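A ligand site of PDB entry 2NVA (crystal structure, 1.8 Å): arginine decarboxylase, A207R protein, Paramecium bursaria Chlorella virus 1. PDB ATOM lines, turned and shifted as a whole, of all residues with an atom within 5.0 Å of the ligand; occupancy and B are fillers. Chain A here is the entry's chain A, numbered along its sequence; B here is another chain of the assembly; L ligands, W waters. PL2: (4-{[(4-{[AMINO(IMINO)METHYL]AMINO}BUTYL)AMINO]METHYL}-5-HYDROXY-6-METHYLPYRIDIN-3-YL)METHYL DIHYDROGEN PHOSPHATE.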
ATOM      1  N   ALA A  46     -10.808   1.907 -18.074  1.00  0.00           N
ATOM      2  CA  ALA A  46      -9.556   2.409 -17.508  1.00  0.00           C
ATOM      3  C   ALA A  46      -8.376   1.713 -18.179  1.00  0.00           C
ATOM      4  O   ALA A  46      -7.991   0.601 -17.813  1.00  0.00           O
ATOM      5  CB  ALA A  46      -9.533   2.212 -15.968  1.00  0.00           C
ATOM      6  N   LYS A  48      -5.288   2.027 -18.067  1.00  0.00           N
ATOM      7  CA  LYS A  48      -4.168   1.675 -17.193  1.00  0.00           C
ATOM      8  C   LYS A  48      -4.200   0.237 -16.705  1.00  0.00           C
ATOM      9  O   LYS A  48      -3.150  -0.318 -16.362  1.00  0.00           O
ATOM     10  CB  LYS A  48      -4.126   2.624 -15.988  1.00  0.00           C
ATOM     11  CG  LYS A  48      -5.409   2.595 -15.165  1.00  0.00           C
ATOM     12  CD  LYS A  48      -5.350   3.478 -13.922  1.00  0.00           C
ATOM     13  CE  LYS A  48      -5.743   4.924 -14.205  1.00  0.00           C
ATOM     14  NZ  LYS A  48      -7.167   5.120 -14.760  1.00  0.00           N
ATOM     15  N   CYS A  49      -5.386  -0.354 -16.648  1.00  0.00           N
ATOM     16  CA  CYS A  49      -5.538  -1.710 -16.127  1.00  0.00           C
ATOM     17  C   CYS A  49      -4.936  -2.761 -17.076  1.00  0.00           C
ATOM     18  O   CYS A  49      -4.344  -3.750 -16.630  1.00  0.00           O
ATOM     19  CB  CYS A  49      -7.013  -1.992 -15.866  1.00  0.00           C
ATOM     20  SG  CYS A  49      -7.351  -3.610 -15.105  1.00  0.00           S
ATOM     21  N   ASP A  67     -11.099   5.937 -20.167  1.00  0.00           N
ATOM     22  CA  ASP A  67     -10.512   6.708 -19.074  1.00  0.00           C
ATOM     23  C   ASP A  67      -9.005   6.630 -19.260  1.00  0.00           C
ATOM     24  O   ASP A  67      -8.409   5.558 -19.100  1.00  0.00           O
ATOM     25  CB  ASP A  67     -10.963   6.121 -17.720  1.00  0.00           C
ATOM     26  CG  ASP A  67      -9.996   6.419 -16.589  1.00  0.00           C
ATOM     27  OD1 ASP A  67     -10.000   5.661 -15.595  1.00  0.00           O
ATOM     28  OD2 ASP A  67      -9.186   7.384 -16.683  1.00  0.00           O
ATOM     29  N   ALA A  90      -9.180  11.165 -16.707  1.00  0.00           N
ATOM     30  CA  ALA A  90      -9.671  10.957 -15.334  1.00  0.00           C
ATOM     31  C   ALA A  90      -8.530  10.830 -14.320  1.00  0.00           C
ATOM     32  O   ALA A  90      -8.452   9.855 -13.566  1.00  0.00           O
ATOM     33  CB  ALA A  90     -10.598   9.737 -15.271  1.00  0.00           C
ATOM     34  N   ARG A 133     -13.718  15.438  -8.409  1.00  0.00           N
ATOM     35  CA  ARG A 133     -13.583  14.154  -7.734  1.00  0.00           C
ATOM     36  C   ARG A 133     -13.641  14.359  -6.224  1.00  0.00           C
ATOM     37  O   ARG A 133     -12.853  15.125  -5.663  1.00  0.00           O
ATOM     38  CB  ARG A 133     -12.288  13.450  -8.113  1.00  0.00           C
ATOM     39  CG  ARG A 133     -12.135  12.095  -7.432  1.00  0.00           C
ATOM     40  CD  ARG A 133     -10.972  11.320  -8.011  1.00  0.00           C
ATOM     41  NE  ARG A 133     -10.671  10.136  -7.197  1.00  0.00           N
ATOM     42  CZ  ARG A 133      -9.686   9.280  -7.485  1.00  0.00           C
ATOM     43  NH1 ARG A 133      -8.924   9.489  -8.550  1.00  0.00           N
ATOM     44  NH2 ARG A 133      -9.464   8.229  -6.707  1.00  0.00           N
ATOM     45  N   VAL A 143      -7.282  -2.053  -2.942  1.00  0.00           N
ATOM     46  CA  VAL A 143      -6.294  -0.972  -3.077  1.00  0.00           C
ATOM     47  C   VAL A 143      -6.954   0.365  -2.710  1.00  0.00           C
ATOM     48  O   VAL A 143      -7.843   0.848  -3.416  1.00  0.00           O
ATOM     49  CB  VAL A 143      -5.696  -0.937  -4.495  1.00  0.00           C
ATOM     50  CG1 VAL A 143      -4.642   0.176  -4.612  1.00  0.00           C
ATOM     51  CG2 VAL A 143      -5.116  -2.320  -4.884  1.00  0.00           C
ATOM     52  N   LEU A 145      -7.340   4.424  -2.165  1.00  0.00           N
ATOM     53  CA  LEU A 145      -7.000   5.576  -3.045  1.00  0.00           C
ATOM     54  C   LEU A 145      -7.284   6.933  -2.418  1.00  0.00           C
ATOM     55  O   LEU A 145      -6.859   7.995  -2.917  1.00  0.00           O
ATOM     56  CB  LEU A 145      -7.789   5.463  -4.365  1.00  0.00           C
ATOM     57  CG  LEU A 145      -7.784   4.187  -5.191  1.00  0.00           C
ATOM     58  CD1 LEU A 145      -8.795   4.291  -6.322  1.00  0.00           C
ATOM     59  CD2 LEU A 145      -6.378   3.838  -5.725  1.00  0.00           C
ATOM     60  N   HIS A 176     -13.955   7.514  -6.585  1.00  0.00           N
ATOM     61  CA  HIS A 176     -13.526   6.135  -6.730  1.00  0.00           C
ATOM     62  C   HIS A 176     -13.417   5.577  -5.320  1.00  0.00           C
ATOM     63  O   HIS A 176     -12.652   6.086  -4.502  1.00  0.00           O
ATOM     64  CB  HIS A 176     -12.174   6.060  -7.445  1.00  0.00           C
ATOM     65  CG  HIS A 176     -11.889   4.698  -8.011  1.00  0.00           C
ATOM     66  ND1 HIS A 176     -12.157   3.540  -7.321  1.00  0.00           N
ATOM     67  CD2 HIS A 176     -11.385   4.315  -9.203  1.00  0.00           C
ATOM     68  CE1 HIS A 176     -11.793   2.496  -8.054  1.00  0.00           C
ATOM     69  NE2 HIS A 176     -11.323   2.940  -9.202  1.00  0.00           N
ATOM     70  N   GLY A 178     -12.216   2.862  -4.355  1.00  0.00           N
ATOM     71  CA  GLY A 178     -11.037   2.038  -4.164  1.00  0.00           C
ATOM     72  C   GLY A 178     -11.032   0.913  -5.181  1.00  0.00           C
ATOM     73  O   GLY A 178     -12.089   0.480  -5.634  1.00  0.00           O
ATOM     74  N   SER A 179      -9.831   0.455  -5.525  1.00  0.00           N
ATOM     75  CA  SER A 179      -9.683  -0.597  -6.523  1.00  0.00           C
ATOM     76  C   SER A 179      -9.911  -1.976  -5.888  1.00  0.00           C
ATOM     77  O   SER A 179      -9.291  -2.306  -4.866  1.00  0.00           O
ATOM     78  CB  SER A 179      -8.299  -0.509  -7.194  1.00  0.00           C
ATOM     79  OG  SER A 179      -8.294  -1.299  -8.394  1.00  0.00           O
ATOM     80  N   GLY A 180     -10.799  -2.768  -6.484  1.00  0.00           N
ATOM     81  CA  GLY A 180     -11.135  -4.093  -5.991  1.00  0.00           C
ATOM     82  C   GLY A 180     -12.123  -3.985  -4.841  1.00  0.00           C
ATOM     83  O   GLY A 180     -11.794  -4.319  -3.690  1.00  0.00           O
ATOM     84  N   GLY A 214     -16.812   5.988 -11.007  1.00  0.00           N
ATOM     85  CA  GLY A 214     -15.442   5.470 -10.898  1.00  0.00           C
ATOM     86  C   GLY A 214     -15.327   3.973 -11.196  1.00  0.00           C
ATOM     87  O   GLY A 214     -16.134   3.442 -11.954  1.00  0.00           O
ATOM     88  N   GLY A 215     -14.331   3.322 -10.597  1.00  0.00           N
ATOM     89  CA  GLY A 215     -14.085   1.888 -10.849  1.00  0.00           C
ATOM     90  C   GLY A 215     -14.251   0.998  -9.616  1.00  0.00           C
ATOM     91  O   GLY A 215     -15.039   1.306  -8.722  1.00  0.00           O
ATOM     92  N   GLY A 216     -13.517  -0.108  -9.604  1.00  0.00           N
ATOM     93  CA  GLY A 216     -13.461  -0.969  -8.432  1.00  0.00           C
ATOM     94  C   GLY A 216     -14.200  -2.290  -8.532  1.00  0.00           C
ATOM     95  O   GLY A 216     -13.894  -3.239  -7.797  1.00  0.00           O
ATOM     96  N   LEU A 217     -15.185  -2.361  -9.418  1.00  0.00           N
ATOM     97  CA  LEU A 217     -16.049  -3.549  -9.513  1.00  0.00           C
ATOM     98  C   LEU A 217     -15.371  -4.754 -10.151  1.00  0.00           C
ATOM     99  O   LEU A 217     -14.621  -4.623 -11.144  1.00  0.00           O
ATOM    100  CB  LEU A 217     -17.331  -3.211 -10.279  1.00  0.00           C
ATOM    101  CG  LEU A 217     -18.214  -2.098  -9.737  1.00  0.00           C
ATOM    102  CD1 LEU A 217     -19.366  -1.874 -10.724  1.00  0.00           C
ATOM    103  CD2 LEU A 217     -18.764  -2.431  -8.360  1.00  0.00           C
ATOM    104  N   GLU A 252     -15.736   4.173 -14.572  1.00  0.00           N
ATOM    105  CA  GLU A 252     -14.362   4.028 -15.021  1.00  0.00           C
ATOM    106  C   GLU A 252     -13.857   2.608 -14.690  1.00  0.00           C
ATOM    107  O   GLU A 252     -12.857   2.460 -13.977  1.00  0.00           O
ATOM    108  CB  GLU A 252     -13.474   5.071 -14.359  1.00  0.00           C
ATOM    109  CG  GLU A 252     -13.919   6.529 -14.581  1.00  0.00           C
ATOM    110  CD  GLU A 252     -13.266   7.507 -13.607  1.00  0.00           C
ATOM    111  OE1 GLU A 252     -12.589   7.065 -12.646  1.00  0.00           O
ATOM    112  OE2 GLU A 252     -13.435   8.735 -13.800  1.00  0.00           O
ATOM    113  N   PRO A 253     -14.556   1.574 -15.196  1.00  0.00           N
ATOM    114  CA  PRO A 253     -14.124   0.230 -14.821  1.00  0.00           C
ATOM    115  C   PRO A 253     -12.819  -0.164 -15.507  1.00  0.00           C
ATOM    116  O   PRO A 253     -12.645   0.111 -16.686  1.00  0.00           O
ATOM    117  CB  PRO A 253     -15.267  -0.668 -15.320  1.00  0.00           C
ATOM    118  CG  PRO A 253     -15.837   0.076 -16.475  1.00  0.00           C
ATOM    119  CD  PRO A 253     -15.708   1.551 -16.124  1.00  0.00           C
ATOM    120  N   GLY A 254     -11.923  -0.814 -14.754  1.00  0.00           N
ATOM    121  CA  GLY A 254     -10.730  -1.408 -15.350  1.00  0.00           C
ATOM    122  C   GLY A 254     -10.837  -2.912 -15.246  1.00  0.00           C
ATOM    123  O   GLY A 254     -11.072  -3.608 -16.243  1.00  0.00           O
ATOM    124  N   ARG A 255     -10.713  -3.418 -14.013  1.00  0.00           N
ATOM    125  CA  ARG A 255     -10.656  -4.855 -13.783  1.00  0.00           C
ATOM    126  C   ARG A 255     -11.931  -5.629 -14.185  1.00  0.00           C
ATOM    127  O   ARG A 255     -11.857  -6.818 -14.442  1.00  0.00           O
ATOM    128  CB  ARG A 255     -10.282  -5.183 -12.322  1.00  0.00           C
ATOM    129  CG  ARG A 255     -11.376  -4.837 -11.307  1.00  0.00           C
ATOM    130  CD  ARG A 255     -10.978  -5.175  -9.882  1.00  0.00           C
ATOM    131  NE  ARG A 255      -9.898  -4.317  -9.381  1.00  0.00           N
ATOM    132  CZ  ARG A 255      -8.661  -4.747  -9.097  1.00  0.00           C
ATOM    133  NH1 ARG A 255      -8.333  -6.032  -9.265  1.00  0.00           N
ATOM    134  NH2 ARG A 255      -7.749  -3.890  -8.654  1.00  0.00           N
ATOM    135  N   PHE A 256     -13.088  -4.951 -14.211  1.00  0.00           N
ATOM    136  CA  PHE A 256     -14.327  -5.623 -14.606  1.00  0.00           C
ATOM    137  C   PHE A 256     -14.175  -6.289 -15.966  1.00  0.00           C
ATOM    138  O   PHE A 256     -14.585  -7.435 -16.151  1.00  0.00           O
ATOM    139  CB  PHE A 256     -15.535  -4.667 -14.605  1.00  0.00           C
ATOM    140  CG  PHE A 256     -16.854  -5.353 -14.895  1.00  0.00           C
ATOM    141  CD1 PHE A 256     -17.663  -5.799 -13.854  1.00  0.00           C
ATOM    142  CD2 PHE A 256     -17.283  -5.546 -16.214  1.00  0.00           C
ATOM    143  CE1 PHE A 256     -18.893  -6.444 -14.131  1.00  0.00           C
ATOM    144  CE2 PHE A 256     -18.497  -6.190 -16.498  1.00  0.00           C
ATOM    145  CZ  PHE A 256     -19.292  -6.635 -15.453  1.00  0.00           C
ATOM    146  N   ASN A 292       0.605  -8.250  -8.708  1.00  0.00           N
ATOM    147  CA  ASN A 292      -0.595  -8.332  -7.852  1.00  0.00           C
ATOM    148  C   ASN A 292      -0.391  -9.130  -6.547  1.00  0.00           C
ATOM    149  O   ASN A 292      -1.140  -8.946  -5.574  1.00  0.00           O
ATOM    150  CB  ASN A 292      -1.799  -8.885  -8.618  1.00  0.00           C
ATOM    151  CG  ASN A 292      -2.435  -7.847  -9.521  1.00  0.00           C
ATOM    152  OD1 ASN A 292      -2.305  -6.642  -9.269  1.00  0.00           O
ATOM    153  ND2 ASN A 292      -3.116  -8.300 -10.593  1.00  0.00           N
ATOM    154  N   PHE A 295       1.002  -6.095  -4.576  1.00  0.00           N
ATOM    155  CA  PHE A 295       0.145  -4.905  -4.422  1.00  0.00           C
ATOM    156  C   PHE A 295      -1.318  -5.196  -4.118  1.00  0.00           C
ATOM    157  O   PHE A 295      -2.033  -4.294  -3.622  1.00  0.00           O
ATOM    158  CB  PHE A 295       0.295  -3.983  -5.624  1.00  0.00           C
ATOM    159  CG  PHE A 295       1.699  -3.451  -5.794  1.00  0.00           C
ATOM    160  CD1 PHE A 295       2.173  -2.424  -4.968  1.00  0.00           C
ATOM    161  CD2 PHE A 295       2.557  -3.991  -6.747  1.00  0.00           C
ATOM    162  CE1 PHE A 295       3.467  -1.933  -5.094  1.00  0.00           C
ATOM    163  CE2 PHE A 295       3.853  -3.514  -6.874  1.00  0.00           C
ATOM    164  CZ  PHE A 295       4.307  -2.476  -6.031  1.00  0.00           C
ATOM    165  N   GLU A 296      -1.796  -6.393  -4.437  1.00  0.00           N
ATOM    166  CA  GLU A 296      -3.212  -6.718  -4.198  1.00  0.00           C
ATOM    167  C   GLU A 296      -3.383  -7.950  -3.309  1.00  0.00           C
ATOM    168  O   GLU A 296      -4.495  -8.478  -3.177  1.00  0.00           O
ATOM    169  CB  GLU A 296      -3.971  -6.900  -5.507  1.00  0.00           C
ATOM    170  CG  GLU A 296      -3.984  -5.666  -6.417  1.00  0.00           C
ATOM    171  CD  GLU A 296      -4.996  -5.746  -7.566  1.00  0.00           C
ATOM    172  OE1 GLU A 296      -5.602  -6.818  -7.798  1.00  0.00           O
ATOM    173  OE2 GLU A 296      -5.202  -4.704  -8.219  1.00  0.00           O
ATOM    174  N   TYR A 353      -4.078  -5.551 -14.239  1.00  0.00           N
ATOM    175  CA  TYR A 353      -2.881  -5.072 -13.523  1.00  0.00           C
ATOM    176  C   TYR A 353      -1.820  -6.175 -13.510  1.00  0.00           C
ATOM    177  O   TYR A 353      -1.222  -6.452 -12.467  1.00  0.00           O
ATOM    178  CB  TYR A 353      -3.233  -4.605 -12.093  1.00  0.00           C
ATOM    179  CG  TYR A 353      -4.300  -3.539 -12.101  1.00  0.00           C
ATOM    180  CD1 TYR A 353      -4.022  -2.262 -12.581  1.00  0.00           C
ATOM    181  CD2 TYR A 353      -5.591  -3.814 -11.665  1.00  0.00           C
ATOM    182  CE1 TYR A 353      -4.990  -1.270 -12.626  1.00  0.00           C
ATOM    183  CE2 TYR A 353      -6.583  -2.832 -11.696  1.00  0.00           C
ATOM    184  CZ  TYR A 353      -6.265  -1.558 -12.188  1.00  0.00           C
ATOM    185  OH  TYR A 353      -7.223  -0.572 -12.241  1.00  0.00           O
ATOM    186  N   LEU A 357       2.276  -3.981 -15.693  1.00  0.00           N
ATOM    187  CA  LEU A 357       3.222  -3.686 -14.629  1.00  0.00           C
ATOM    188  C   LEU A 357       4.568  -4.430 -14.742  1.00  0.00           C
ATOM    189  O   LEU A 357       5.333  -4.517 -13.778  1.00  0.00           O
ATOM    190  CB  LEU A 357       2.572  -3.953 -13.277  1.00  0.00           C
ATOM    191  CG  LEU A 357       1.697  -2.773 -12.850  1.00  0.00           C
ATOM    192  CD1 LEU A 357       0.508  -3.261 -12.072  1.00  0.00           C
ATOM    193  CD2 LEU A 357       2.517  -1.798 -12.035  1.00  0.00           C
ATOM    194  N   TYR B 287       6.296   3.427  -9.179  1.00  0.00           N
ATOM    195  CA  TYR B 287       6.285   2.519 -10.343  1.00  0.00           C
ATOM    196  C   TYR B 287       7.272   2.946 -11.428  1.00  0.00           C
ATOM    197  O   TYR B 287       7.423   2.254 -12.462  1.00  0.00           O
ATOM    198  CB  TYR B 287       4.868   2.433 -10.924  1.00  0.00           C
ATOM    199  CG  TYR B 287       3.876   1.783  -9.985  1.00  0.00           C
ATOM    200  CD1 TYR B 287       3.832   0.402  -9.834  1.00  0.00           C
ATOM    201  CD2 TYR B 287       2.947   2.552  -9.282  1.00  0.00           C
ATOM    202  CE1 TYR B 287       2.903  -0.207  -8.990  1.00  0.00           C
ATOM    203  CE2 TYR B 287       2.000   1.941  -8.422  1.00  0.00           C
ATOM    204  CZ  TYR B 287       1.989   0.563  -8.294  1.00  0.00           C
ATOM    205  OH  TYR B 287       1.057  -0.066  -7.463  1.00  0.00           O
ATOM    206  N   CYS B 324      -2.188   6.740 -10.432  1.00  0.00           N
ATOM    207  CA  CYS B 324      -3.495   6.766  -9.773  1.00  0.00           C
ATOM    208  C   CYS B 324      -3.578   5.866  -8.523  1.00  0.00           C
ATOM    209  O   CYS B 324      -4.630   5.798  -7.879  1.00  0.00           O
ATOM    210  CB  CYS B 324      -4.587   6.391 -10.785  1.00  0.00           C
ATOM    211  SG  CYS B 324      -4.836   7.605 -12.089  1.00  0.00           S
ATOM    212  N   ASP B 325      -2.472   5.194  -8.178  1.00  0.00           N
ATOM    213  CA  ASP B 325      -2.439   4.304  -7.024  1.00  0.00           C
ATOM    214  C   ASP B 325      -2.156   4.998  -5.698  1.00  0.00           C
ATOM    215  O   ASP B 325      -1.249   5.826  -5.609  1.00  0.00           O
ATOM    216  CB  ASP B 325      -1.365   3.223  -7.263  1.00  0.00           C
ATOM    217  CG  ASP B 325      -1.600   1.970  -6.442  1.00  0.00           C
ATOM    218  OD1 ASP B 325      -1.988   2.062  -5.243  1.00  0.00           O
ATOM    219  OD2 ASP B 325      -1.384   0.865  -6.988  1.00  0.00           O
ATOM    220  N   PHE B 361       3.493   1.766 -16.125  1.00  0.00           N
ATOM    221  CA  PHE B 361       2.164   1.774 -15.525  1.00  0.00           C
ATOM    222  C   PHE B 361       1.563   3.186 -15.590  1.00  0.00           C
ATOM    223  O   PHE B 361       2.256   4.177 -15.337  1.00  0.00           O
ATOM    224  CB  PHE B 361       2.232   1.268 -14.078  1.00  0.00           C
ATOM    225  CG  PHE B 361       0.895   1.063 -13.419  1.00  0.00           C
ATOM    226  CD1 PHE B 361      -0.145   0.422 -14.085  1.00  0.00           C
ATOM    227  CD2 PHE B 361       0.692   1.486 -12.094  1.00  0.00           C
ATOM    228  CE1 PHE B 361      -1.377   0.242 -13.451  1.00  0.00           C
ATOM    229  CE2 PHE B 361      -0.538   1.307 -11.470  1.00  0.00           C
ATOM    230  CZ  PHE B 361      -1.567   0.675 -12.153  1.00  0.00           C
HETATM  231  N1  PL2 L   1     -10.570   5.126 -12.584  1.00  0.00           N
HETATM  232  C2  PL2 L   1      -9.567   5.700 -11.902  1.00  0.00           C
HETATM  233  C2A PL2 L   1      -9.436   7.236 -11.864  1.00  0.00           C
HETATM  234  C3  PL2 L   1      -8.650   4.880 -11.234  1.00  0.00           C
HETATM  235  O3  PL2 L   1      -7.658   5.487 -10.540  1.00  0.00           O
HETATM  236  C4  PL2 L   1      -8.761   3.473 -11.265  1.00  0.00           C
HETATM  237  C4A PL2 L   1      -7.753   2.521 -10.548  1.00  0.00           C
HETATM  238  C5  PL2 L   1      -9.835   2.948 -11.999  1.00  0.00           C
HETATM  239  C6  PL2 L   1     -10.715   3.797 -12.646  1.00  0.00           C
HETATM  240  P   PL2 L   1     -10.641  -0.803 -11.245  1.00  0.00           P
HETATM  241  N   PL2 L   1      -7.114   3.153  -9.365  1.00  0.00           N
HETATM  242  CA  PL2 L   1      -5.716   2.718  -9.210  1.00  0.00           C
HETATM  243  CG  PL2 L   1      -4.171   0.747  -8.846  1.00  0.00           C
HETATM  244  OP2 PL2 L   1     -10.586  -1.537  -9.813  1.00  0.00           O
HETATM  245  OP3 PL2 L   1      -9.574  -1.577 -12.196  1.00  0.00           O
HETATM  246  OP1 PL2 L   1     -12.029  -0.810 -11.813  1.00  0.00           O
HETATM  247  OP4 PL2 L   1     -10.068   0.665 -10.930  1.00  0.00           O
HETATM  248  C5M PL2 L   1     -10.057   1.424 -12.087  1.00  0.00           C
HETATM  249  CB  PL2 L   1      -5.619   1.187  -9.104  1.00  0.00           C
HETATM  250  CD  PL2 L   1      -4.069  -0.787  -8.698  1.00  0.00           C
HETATM  251  NE  PL2 L   1      -2.632  -1.091  -8.552  1.00  0.00           N
HETATM  252  CZ  PL2 L   1      -2.073  -2.305  -8.672  1.00  0.00           C
HETATM  253  NH2 PL2 L   1      -0.728  -2.424  -8.518  1.00  0.00           N
HETATM  254  NH1 PL2 L   1      -2.817  -3.385  -8.935  1.00  0.00           N
HETATM  255  O   HOH W   1      -7.170   7.092  -8.265  1.00  0.00           O
HETATM  256  O   HOH W   2     -14.157  -2.315 -12.561  1.00  0.00           O
HETATM  257  O   HOH W   3      -0.150  -5.129  -9.183  1.00  0.00           O
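A nitrogen (N1) of the ligand lies close to the side-chain carboxylate (OD1) of Asp 67, at 3.1 Å.
Merely in contact with the ligand: Ala 46, Lys 48, Ala 90, Leu 145, Gly 180, Gly 215, Pro 253, Phe 295, Leu 357 and Cys 324 of chain B.
The nearest printed residue that does not touch the ligand is Arg 133 (4.04 Å).
Water W2 lies within hydrogen-bond range of OP1 of the ligand (2.7 Å), O of Leu 217 (2.7 Å), N of Phe 256 (3.3 Å) and N of Gly 254 (3.5 Å).
Water W1 lies within hydrogen-bond range of O3 of the ligand, O of Cys 324 of chain B and NH1 of Arg 133.
Water W3 lies within hydrogen-bond range of the side-chain amide oxygen (OD1) of Asn 292 (2.6 Å) and a nitrogen (NH2) of the ligand (2.8 Å).
The backbone NH of Tyr 353 sits at hydrogen-bond distance from the backbone carbonyl oxygen of Cys 49, at 3.0 Å.
N of Gly 215 sits at hydrogen-bond distance from NE2 of His 176 (3.3 Å).
O of Tyr 353 lies within hydrogen-bond range of ND2 of Asn 292, 3.2 Å away.
The backbone carbonyl oxygen of Gly 216 is in hydrogen-bond range of the backbone NH of Gly 180, 3.4 Å away.
The side-chain carboxylate of Asp 67 is in salt-bridge range of the side-chain amino group of Lys 48 (3.0 Å).
NH2 of Arg 255 is in salt-bridge range of OE2 of Glu 296.
N of Ala 46 lies within hydrogen-bond range of O of Pro 253 (2.9 Å).
The backbone NH (N) of Arg 255 lies within hydrogen-bond range of the side-chain sulfur (SG) of Cys 49, 3.5 Å away.
An oxygen (OP2) of the ligand is in salt-bridge range of the guanidinium group (NE) of Arg 255 (2.9 Å).
OE2 of Glu 296 is in salt-bridge range of NH1 of the ligand (2.8 Å).
The backbone NH of Arg 255 sits at hydrogen-bond distance from an oxygen (OP3) of the ligand.
The side-chain hydroxyl (OH) of Tyr 353 sits at hydrogen-bond distance from an oxygen (OP3) of the ligand (2.6 Å).
OD1 of Asn 292 sits at hydrogen-bond distance from NH1 of the ligand (3.3 Å).
An oxygen (OP1) of the ligand sits at hydrogen-bond distance from the backbone NH (N) of Gly 216 (2.8 Å).
N1 of the ligand sits at hydrogen-bond distance from OE1 of Glu 252 (2.8 Å).
N of Gly 254 sits at hydrogen-bond distance from OP1 of the ligand, 2.9 Å away.
A ring nitrogen (NE2) of His 176 lies within hydrogen-bond range of an oxygen (OP4) of the ligand (3.1 Å).
The side-chain hydroxyl of Tyr 287 of chain B is in hydrogen-bond range of a nitrogen (NH2) of the ligand (3.1 Å).
OD2 of Asp 325 of chain B lies within salt-bridge range of NE of the ligand.
An oxygen (OP2) of the ligand is in hydrogen-bond range of the side-chain hydroxyl (OG) of Ser 179, 2.7 Å away.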
